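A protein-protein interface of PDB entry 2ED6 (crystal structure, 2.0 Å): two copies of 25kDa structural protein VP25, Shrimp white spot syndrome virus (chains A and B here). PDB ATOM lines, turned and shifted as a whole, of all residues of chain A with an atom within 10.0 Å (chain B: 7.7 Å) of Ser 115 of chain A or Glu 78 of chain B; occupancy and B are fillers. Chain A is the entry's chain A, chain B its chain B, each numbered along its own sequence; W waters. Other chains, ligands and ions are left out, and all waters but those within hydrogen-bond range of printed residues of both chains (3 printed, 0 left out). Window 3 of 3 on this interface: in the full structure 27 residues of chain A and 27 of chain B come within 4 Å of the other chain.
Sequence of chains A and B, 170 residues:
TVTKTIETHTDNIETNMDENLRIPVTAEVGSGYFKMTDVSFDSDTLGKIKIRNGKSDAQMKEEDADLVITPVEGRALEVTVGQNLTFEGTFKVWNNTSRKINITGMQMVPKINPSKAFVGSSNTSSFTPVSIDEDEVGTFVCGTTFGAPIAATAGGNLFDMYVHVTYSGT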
ATOM      1  N   LYS A 111      12.081  36.234 -23.665  1.00  0.00           N
ATOM      2  CA  LYS A 111      12.603  34.937 -23.246  1.00  0.00           C
ATOM      3  C   LYS A 111      11.508  33.877 -23.142  1.00  0.00           C
ATOM      4  O   LYS A 111      10.451  34.116 -22.565  1.00  0.00           O
ATOM      5  CB  LYS A 111      13.319  35.066 -21.898  1.00  0.00           C
ATOM      6  CG  LYS A 111      13.964  33.775 -21.423  1.00  0.00           C
ATOM      7  CD  LYS A 111      14.669  33.965 -20.089  1.00  0.00           C
ATOM      8  CE  LYS A 111      15.336  32.680 -19.629  1.00  0.00           C
ATOM      9  NZ  LYS A 111      16.005  32.847 -18.306  1.00  0.00           N
ATOM     10  N   ILE A 112      11.762  32.707 -23.714  1.00  0.00           N
ATOM     11  CA  ILE A 112      10.796  31.615 -23.657  1.00  0.00           C
ATOM     12  C   ILE A 112      10.835  31.075 -22.232  1.00  0.00           C
ATOM     13  O   ILE A 112      11.904  30.715 -21.740  1.00  0.00           O
ATOM     14  CB  ILE A 112      11.174  30.502 -24.659  1.00  0.00           C
ATOM     15  CG1 ILE A 112      11.165  31.074 -26.081  1.00  0.00           C
ATOM     16  CG2 ILE A 112      10.198  29.327 -24.542  1.00  0.00           C
ATOM     17  CD1 ILE A 112      11.713  30.142 -27.134  1.00  0.00           C
ATOM     18  N   ASN A 113       9.684  31.032 -21.563  1.00  0.00           N
ATOM     19  CA  ASN A 113       9.647  30.554 -20.186  1.00  0.00           C
ATOM     20  C   ASN A 113       9.586  29.034 -20.074  1.00  0.00           C
ATOM     21  O   ASN A 113       9.476  28.329 -21.084  1.00  0.00           O
ATOM     22  CB  ASN A 113       8.474  31.193 -19.417  1.00  0.00           C
ATOM     23  CG  ASN A 113       7.111  30.723 -19.901  1.00  0.00           C
ATOM     24  OD1 ASN A 113       6.975  29.655 -20.499  1.00  0.00           O
ATOM     25  ND2 ASN A 113       6.081  31.523 -19.619  1.00  0.00           N
ATOM     26  N   PRO A 114       9.675  28.504 -18.840  1.00  0.00           N
ATOM     27  CA  PRO A 114       9.627  27.055 -18.628  1.00  0.00           C
ATOM     28  C   PRO A 114       8.365  26.407 -19.185  1.00  0.00           C
ATOM     29  O   PRO A 114       8.365  25.222 -19.513  1.00  0.00           O
ATOM     30  CB  PRO A 114       9.722  26.927 -17.108  1.00  0.00           C
ATOM     31  CG  PRO A 114      10.600  28.085 -16.741  1.00  0.00           C
ATOM     32  CD  PRO A 114      10.014  29.201 -17.583  1.00  0.00           C
ATOM     33  N   SER A 115       7.289  27.184 -19.282  1.00  0.00           N
ATOM     34  CA  SER A 115       6.028  26.678 -19.806  1.00  0.00           C
ATOM     35  C   SER A 115       5.991  26.766 -21.328  1.00  0.00           C
ATOM     36  O   SER A 115       4.948  26.560 -21.946  1.00  0.00           O
ATOM     37  CB  SER A 115       4.855  27.458 -19.217  1.00  0.00           C
ATOM     38  OG  SER A 115       4.758  27.231 -17.822  1.00  0.00           O
ATOM     39  N   LYS A 116       7.135  27.092 -21.922  1.00  0.00           N
ATOM     40  CA  LYS A 116       7.264  27.183 -23.372  1.00  0.00           C
ATOM     41  C   LYS A 116       6.454  28.299 -24.028  1.00  0.00           C
ATOM     42  O   LYS A 116       6.004  28.162 -25.169  1.00  0.00           O
ATOM     43  CB  LYS A 116       6.904  25.835 -24.004  1.00  0.00           C
ATOM     44  CG  LYS A 116       7.718  24.671 -23.445  1.00  0.00           C
ATOM     45  CD  LYS A 116       7.496  23.380 -24.224  1.00  0.00           C
ATOM     46  CE  LYS A 116       6.039  22.966 -24.218  1.00  0.00           C
ATOM     47  NZ  LYS A 116       5.523  22.755 -22.837  1.00  0.00           N
ATOM     48  N   ALA A 117       6.281  29.404 -23.316  1.00  0.00           N
ATOM     49  CA  ALA A 117       5.540  30.544 -23.842  1.00  0.00           C
ATOM     50  C   ALA A 117       6.441  31.769 -23.817  1.00  0.00           C
ATOM     51  O   ALA A 117       7.445  31.788 -23.107  1.00  0.00           O
ATOM     52  CB  ALA A 117       4.293  30.799 -22.992  1.00  0.00           C
ATOM     53  N   PHE A 118       6.083  32.786 -24.593  1.00  0.00           N
ATOM     54  CA  PHE A 118       6.854  34.023 -24.628  1.00  0.00           C
ATOM     55  C   PHE A 118       5.940  35.197 -24.975  1.00  0.00           C
ATOM     56  O   PHE A 118       4.926  35.021 -25.644  1.00  0.00           O
ATOM     57  CB  PHE A 118       8.012  33.904 -25.632  1.00  0.00           C
ATOM     58  CG  PHE A 118       7.580  33.795 -27.073  1.00  0.00           C
ATOM     59  CD1 PHE A 118       7.440  34.935 -27.861  1.00  0.00           C
ATOM     60  CD2 PHE A 118       7.348  32.552 -27.650  1.00  0.00           C
ATOM     61  CE1 PHE A 118       7.076  34.838 -29.212  1.00  0.00           C
ATOM     62  CE2 PHE A 118       6.985  32.437 -28.997  1.00  0.00           C
ATOM     63  CZ  PHE A 118       6.849  33.583 -29.781  1.00  0.00           C
ATOM     64  N   VAL A 119       6.284  36.385 -24.499  1.00  0.00           N
ATOM     65  CA  VAL A 119       5.481  37.576 -24.767  1.00  0.00           C
ATOM     66  C   VAL A 119       5.544  37.880 -26.258  1.00  0.00           C
ATOM     67  O   VAL A 119       6.608  38.231 -26.783  1.00  0.00           O
ATOM     68  CB  VAL A 119       6.012  38.790 -23.969  1.00  0.00           C
ATOM     69  CG1 VAL A 119       5.206  40.044 -24.317  1.00  0.00           C
ATOM     70  CG2 VAL A 119       5.931  38.503 -22.479  1.00  0.00           C
ATOM     71  N   GLY A 120       4.404  37.750 -26.930  1.00  0.00           N
ATOM     72  CA  GLY A 120       4.354  37.982 -28.363  1.00  0.00           C
ATOM     73  C   GLY A 120       3.628  39.216 -28.868  1.00  0.00           C
ATOM     74  O   GLY A 120       3.199  39.250 -30.020  1.00  0.00           O
ATOM     75  N   THR A 153       4.750  38.362 -14.310  1.00  0.00           N
ATOM     76  CA  THR A 153       4.048  37.090 -14.363  1.00  0.00           C
ATOM     77  C   THR A 153       4.565  36.199 -15.493  1.00  0.00           C
ATOM     78  O   THR A 153       4.781  36.660 -16.611  1.00  0.00           O
ATOM     79  CB  THR A 153       2.536  37.302 -14.570  1.00  0.00           C
ATOM     80  OG1 THR A 153       2.055  38.260 -13.620  1.00  0.00           O
ATOM     81  CG2 THR A 153       1.784  35.992 -14.386  1.00  0.00           C
ATOM     82  N   ALA A 154       4.760  34.920 -15.184  1.00  0.00           N
ATOM     83  CA  ALA A 154       5.231  33.928 -16.150  1.00  0.00           C
ATOM     84  C   ALA A 154       6.524  34.329 -16.859  1.00  0.00           C
ATOM     85  O   ALA A 154       6.730  33.994 -18.030  1.00  0.00           O
ATOM     86  CB  ALA A 154       4.138  33.651 -17.179  1.00  0.00           C
ATOM     87  N   GLY A 155       7.393  35.039 -16.142  1.00  0.00           N
ATOM     88  CA  GLY A 155       8.654  35.478 -16.717  1.00  0.00           C
ATOM     89  C   GLY A 155       8.447  36.443 -17.872  1.00  0.00           C
ATOM     90  O   GLY A 155       9.306  36.576 -18.745  1.00  0.00           O
ATOM     91  N   ARG B  75       6.949  20.285 -30.432  1.00  0.00           N
ATOM     92  CA  ARG B  75       6.161  21.222 -29.645  1.00  0.00           C
ATOM     93  C   ARG B  75       6.995  21.855 -28.534  1.00  0.00           C
ATOM     94  O   ARG B  75       6.610  21.819 -27.360  1.00  0.00           O
ATOM     95  CB  ARG B  75       4.949  20.506 -29.038  1.00  0.00           C
ATOM     96  CG  ARG B  75       3.788  21.415 -28.625  1.00  0.00           C
ATOM     97  CD  ARG B  75       3.007  21.929 -29.841  1.00  0.00           C
ATOM     98  NE  ARG B  75       3.743  22.954 -30.576  1.00  0.00           N
ATOM     99  CZ  ARG B  75       3.452  23.349 -31.811  1.00  0.00           C
ATOM    100  NH1 ARG B  75       2.433  22.801 -32.465  1.00  0.00           N
ATOM    101  NH2 ARG B  75       4.180  24.296 -32.394  1.00  0.00           N
ATOM    102  N   ALA B  76       8.140  22.428 -28.899  1.00  0.00           N
ATOM    103  CA  ALA B  76       9.010  23.084 -27.924  1.00  0.00           C
ATOM    104  C   ALA B  76       8.399  24.436 -27.581  1.00  0.00           C
ATOM    105  O   ALA B  76       8.869  25.154 -26.705  1.00  0.00           O
ATOM    106  CB  ALA B  76      10.406  23.265 -28.500  1.00  0.00           C
ATOM    107  N   LEU B  77       7.332  24.775 -28.289  1.00  0.00           N
ATOM    108  CA  LEU B  77       6.624  26.023 -28.071  1.00  0.00           C
ATOM    109  C   LEU B  77       5.155  25.688 -27.824  1.00  0.00           C
ATOM    110  O   LEU B  77       4.544  24.940 -28.590  1.00  0.00           O
ATOM    111  CB  LEU B  77       6.766  26.927 -29.304  1.00  0.00           C
ATOM    112  CG  LEU B  77       7.518  28.258 -29.181  1.00  0.00           C
ATOM    113  CD1 LEU B  77       8.750  28.110 -28.302  1.00  0.00           C
ATOM    114  CD2 LEU B  77       7.895  28.748 -30.577  1.00  0.00           C
ATOM    115  N   GLU B  78       4.605  26.229 -26.746  1.00  0.00           N
ATOM    116  CA  GLU B  78       3.208  26.013 -26.377  1.00  0.00           C
ATOM    117  C   GLU B  78       2.303  26.819 -27.311  1.00  0.00           C
ATOM    118  O   GLU B  78       2.455  28.039 -27.427  1.00  0.00           O
ATOM    119  CB  GLU B  78       2.983  26.466 -24.937  1.00  0.00           C
ATOM    120  CG  GLU B  78       1.530  26.496 -24.508  1.00  0.00           C
ATOM    121  CD  GLU B  78       1.321  27.306 -23.242  1.00  0.00           C
ATOM    122  OE1 GLU B  78       1.905  26.944 -22.198  1.00  0.00           O
ATOM    123  OE2 GLU B  78       0.578  28.308 -23.293  1.00  0.00           O
ATOM    124  N   VAL B  79       1.352  26.153 -27.961  1.00  0.00           N
ATOM    125  CA  VAL B  79       0.472  26.857 -28.892  1.00  0.00           C
ATOM    126  C   VAL B  79      -0.931  26.263 -28.997  1.00  0.00           C
ATOM    127  O   VAL B  79      -1.118  25.067 -28.810  1.00  0.00           O
ATOM    128  CB  VAL B  79       1.080  26.854 -30.324  1.00  0.00           C
ATOM    129  CG1 VAL B  79       0.148  27.533 -31.278  1.00  0.00           C
ATOM    130  CG2 VAL B  79       2.428  27.549 -30.333  1.00  0.00           C
ATOM    131  N   THR B  80      -1.915  27.114 -29.283  1.00  0.00           N
ATOM    132  CA  THR B  80      -3.283  26.656 -29.487  1.00  0.00           C
ATOM    133  C   THR B  80      -3.415  26.684 -31.009  1.00  0.00           C
ATOM    134  O   THR B  80      -3.712  27.716 -31.611  1.00  0.00           O
ATOM    135  CB  THR B  80      -4.321  27.600 -28.849  1.00  0.00           C
ATOM    136  OG1 THR B  80      -4.172  27.575 -27.425  1.00  0.00           O
ATOM    137  CG2 THR B  80      -5.741  27.156 -29.209  1.00  0.00           C
ATOM    138  N   VAL B  81      -3.146  25.534 -31.614  1.00  0.00           N
ATOM    139  CA  VAL B  81      -3.158  25.336 -33.057  1.00  0.00           C
ATOM    140  C   VAL B  81      -4.263  26.007 -33.879  1.00  0.00           C
ATOM    141  O   VAL B  81      -3.998  26.546 -34.959  1.00  0.00           O
ATOM    142  CB  VAL B  81      -3.133  23.815 -33.347  1.00  0.00           C
ATOM    143  CG1 VAL B  81      -3.763  23.515 -34.673  1.00  0.00           C
ATOM    144  CG2 VAL B  81      -1.693  23.319 -33.311  1.00  0.00           C
ATOM    145  N   THR B  86       0.596  31.749 -33.412  1.00  0.00           N
ATOM    146  CA  THR B  86       1.983  31.398 -33.121  1.00  0.00           C
ATOM    147  C   THR B  86       2.438  30.141 -33.858  1.00  0.00           C
ATOM    148  O   THR B  86       1.781  29.104 -33.788  1.00  0.00           O
ATOM    149  CB  THR B  86       2.176  31.168 -31.606  1.00  0.00           C
ATOM    150  OG1 THR B  86       1.872  32.377 -30.902  1.00  0.00           O
ATOM    151  CG2 THR B  86       3.613  30.747 -31.304  1.00  0.00           C
ATOM    152  N   PHE B  87       3.561  30.240 -34.564  1.00  0.00           N
ATOM    153  CA  PHE B  87       4.101  29.100 -35.300  1.00  0.00           C
ATOM    154  C   PHE B  87       5.531  28.796 -34.873  1.00  0.00           C
ATOM    155  O   PHE B  87       6.327  29.703 -34.631  1.00  0.00           O
ATOM    156  CB  PHE B  87       4.035  29.352 -36.810  1.00  0.00           C
ATOM    157  CG  PHE B  87       2.629  29.416 -37.346  1.00  0.00           C
ATOM    158  CD1 PHE B  87       1.851  30.563 -37.177  1.00  0.00           C
ATOM    159  CD2 PHE B  87       2.070  28.317 -37.983  1.00  0.00           C
ATOM    160  CE1 PHE B  87       0.536  30.608 -37.638  1.00  0.00           C
ATOM    161  CE2 PHE B  87       0.759  28.351 -38.445  1.00  0.00           C
ATOM    162  CZ  PHE B  87      -0.012  29.498 -38.272  1.00  0.00           C
ATOM    163  N   GLU B  88       5.845  27.509 -34.779  1.00  0.00           N
ATOM    164  CA  GLU B  88       7.159  27.050 -34.349  1.00  0.00           C
ATOM    165  C   GLU B  88       8.021  26.642 -35.530  1.00  0.00           C
ATOM    166  O   GLU B  88       7.550  25.940 -36.430  1.00  0.00           O
ATOM    167  CB  GLU B  88       6.999  25.860 -33.389  1.00  0.00           C
ATOM    168  CG  GLU B  88       8.307  25.316 -32.820  1.00  0.00           C
ATOM    169  CD  GLU B  88       8.078  24.254 -31.743  1.00  0.00           C
ATOM    170  OE1 GLU B  88       6.919  24.090 -31.291  1.00  0.00           O
ATOM    171  OE2 GLU B  88       9.058  23.586 -31.345  1.00  0.00           O
ATOM    172  N   THR B 145       5.118  34.922 -33.230  1.00  0.00           N
ATOM    173  CA  THR B 145       3.725  35.190 -32.912  1.00  0.00           C
ATOM    174  C   THR B 145       3.305  36.419 -33.720  1.00  0.00           C
ATOM    175  O   THR B 145       4.009  37.438 -33.739  1.00  0.00           O
ATOM    176  CB  THR B 145       3.525  35.446 -31.396  1.00  0.00           C
ATOM    177  OG1 THR B 145       3.723  34.219 -30.680  1.00  0.00           O
ATOM    178  CG2 THR B 145       2.111  35.950 -31.120  1.00  0.00           C
HETATM  179  O   HOH W   1       4.592  29.304 -27.492  1.00  0.00           O
HETATM  180  O   HOH W   2       2.972  39.848 -32.842  1.00  0.00           O
HETATM  181  O   HOH W   3       3.634  34.589 -28.089  1.00  0.00           O
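Water W1 lies within hydrogen-bond range of O of Glu 78 of chain B and O of Lys 116 of chain A. Water W3 lies within hydrogen-bond range of the side-chain hydroxyl (OG1) of Thr 145 of chain B (2.6 Å), the backbone carbonyl oxygen (O) of Phe 118 of chain A (2.8 Å) and the backbone NH (N) of Gly 120 of chain A (3.5 Å). Water W2 bridges O of Thr 145 of chain B and O of Gly 120 of chain A.
Hydrophobic or aromatic side chains of chain A within 4 Å of the printed part of chain B: Ile 112 and Phe 118. Of the 11 printed residues of chain B, 5 touch a printed residue of chain A. Hydrophobic or aromatic side chains of chain B that line the printed part of chain A: Leu 77. Among the printed residues, no Asp or Glu carboxylate lies within 4 Å of a Lys or Arg side-chain nitrogen of the other chain.
The backbone carbonyl oxygen of Lys 116 of chain A lies within hydrogen-bond range of the backbone NH of Glu 78 of chain B, at 2.9 Å. The backbone carbonyl oxygen (O) of Ser 115 of chain A sits close to the side-chain carboxylate (OE1) of Glu 78 of chain B.
No position is printed for both chains. Of the 8 pairs that touch across the chains among the printed residues, none has its exchanged pair printed and touching as well.
The side-chain amide oxygen of Asn 113 of chain A lies within hydrogen-bond range of the backbone NH of Ser 115 of chain A (2.8 Å). The side-chain amide oxygen of Asn 113 of chain A lies within hydrogen-bond range of the backbone NH of Lys 116 of chain A (2.9 Å). The guanidinium group (NH2) of Arg 75 of chain B lies within salt-bridge range of the side-chain carboxylate (OE1) of Glu 88 of chain B, 3.0 Å away. OE2 of Glu 88 of chain B is in hydrogen-bond range of N of Ala 76 of chain B (2.9 Å). The side-chain carboxylate (OE1) of Glu 88 of chain B lies within hydrogen-bond range of the backbone NH (N) of Leu 77 of chain B. The side-chain hydroxyl (OG1) of Thr 145 of chain B sits at hydrogen-bond distance from the side-chain hydroxyl (OG1) of Thr 86 of chain B, at 2.6 Å.
Of chain B, only Glu 78 (3.1 Å) comes within 4 Å of Ser 115 of chain A. Glu 78 of chain B touches just these residues of chain A: Ser 115 and Lys 116. Of chain A, only Ile 112 (3.8 Å) and Lys 116 (3.7 Å) come within 4 Å of Leu 77 of chain B. Of the printed residues of chain B, Phe 118 of chain A touches Thr 145. Printed residues of chain B within 4 Å of Lys 116 of chain A: Arg 75 (3.4 Å), Ala 76 (3.3 Å), Leu 77 (3.7 Å) and Glu 78 (2.9 Å). Printed residues of chain A within 4 Å of Arg 75 of chain B: Lys 116. Thr 153 of chain A touches none of the printed residues of chain B. Gly 155 of chain A touches none of the printed residues of chain B. The nearest residue of chain B that does not touch Ser 115 of chain A is Leu 77 of chain B (5.9 Å).
Leu 77 of chain B touches Ile 112 of chain A. CE of Lys 116 of chain A touches O of Arg 75 of chain B, 3.4 Å away. Lys 116 of chain A touches Ala 76 of chain B (CD to O, 3.3 Å). Leu 77 of chain B touches Lys 116 of chain A. Phe 118 of chain A touches Thr 145 of chain B. Gly 120 of chain A touches Thr 145 of chain B.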
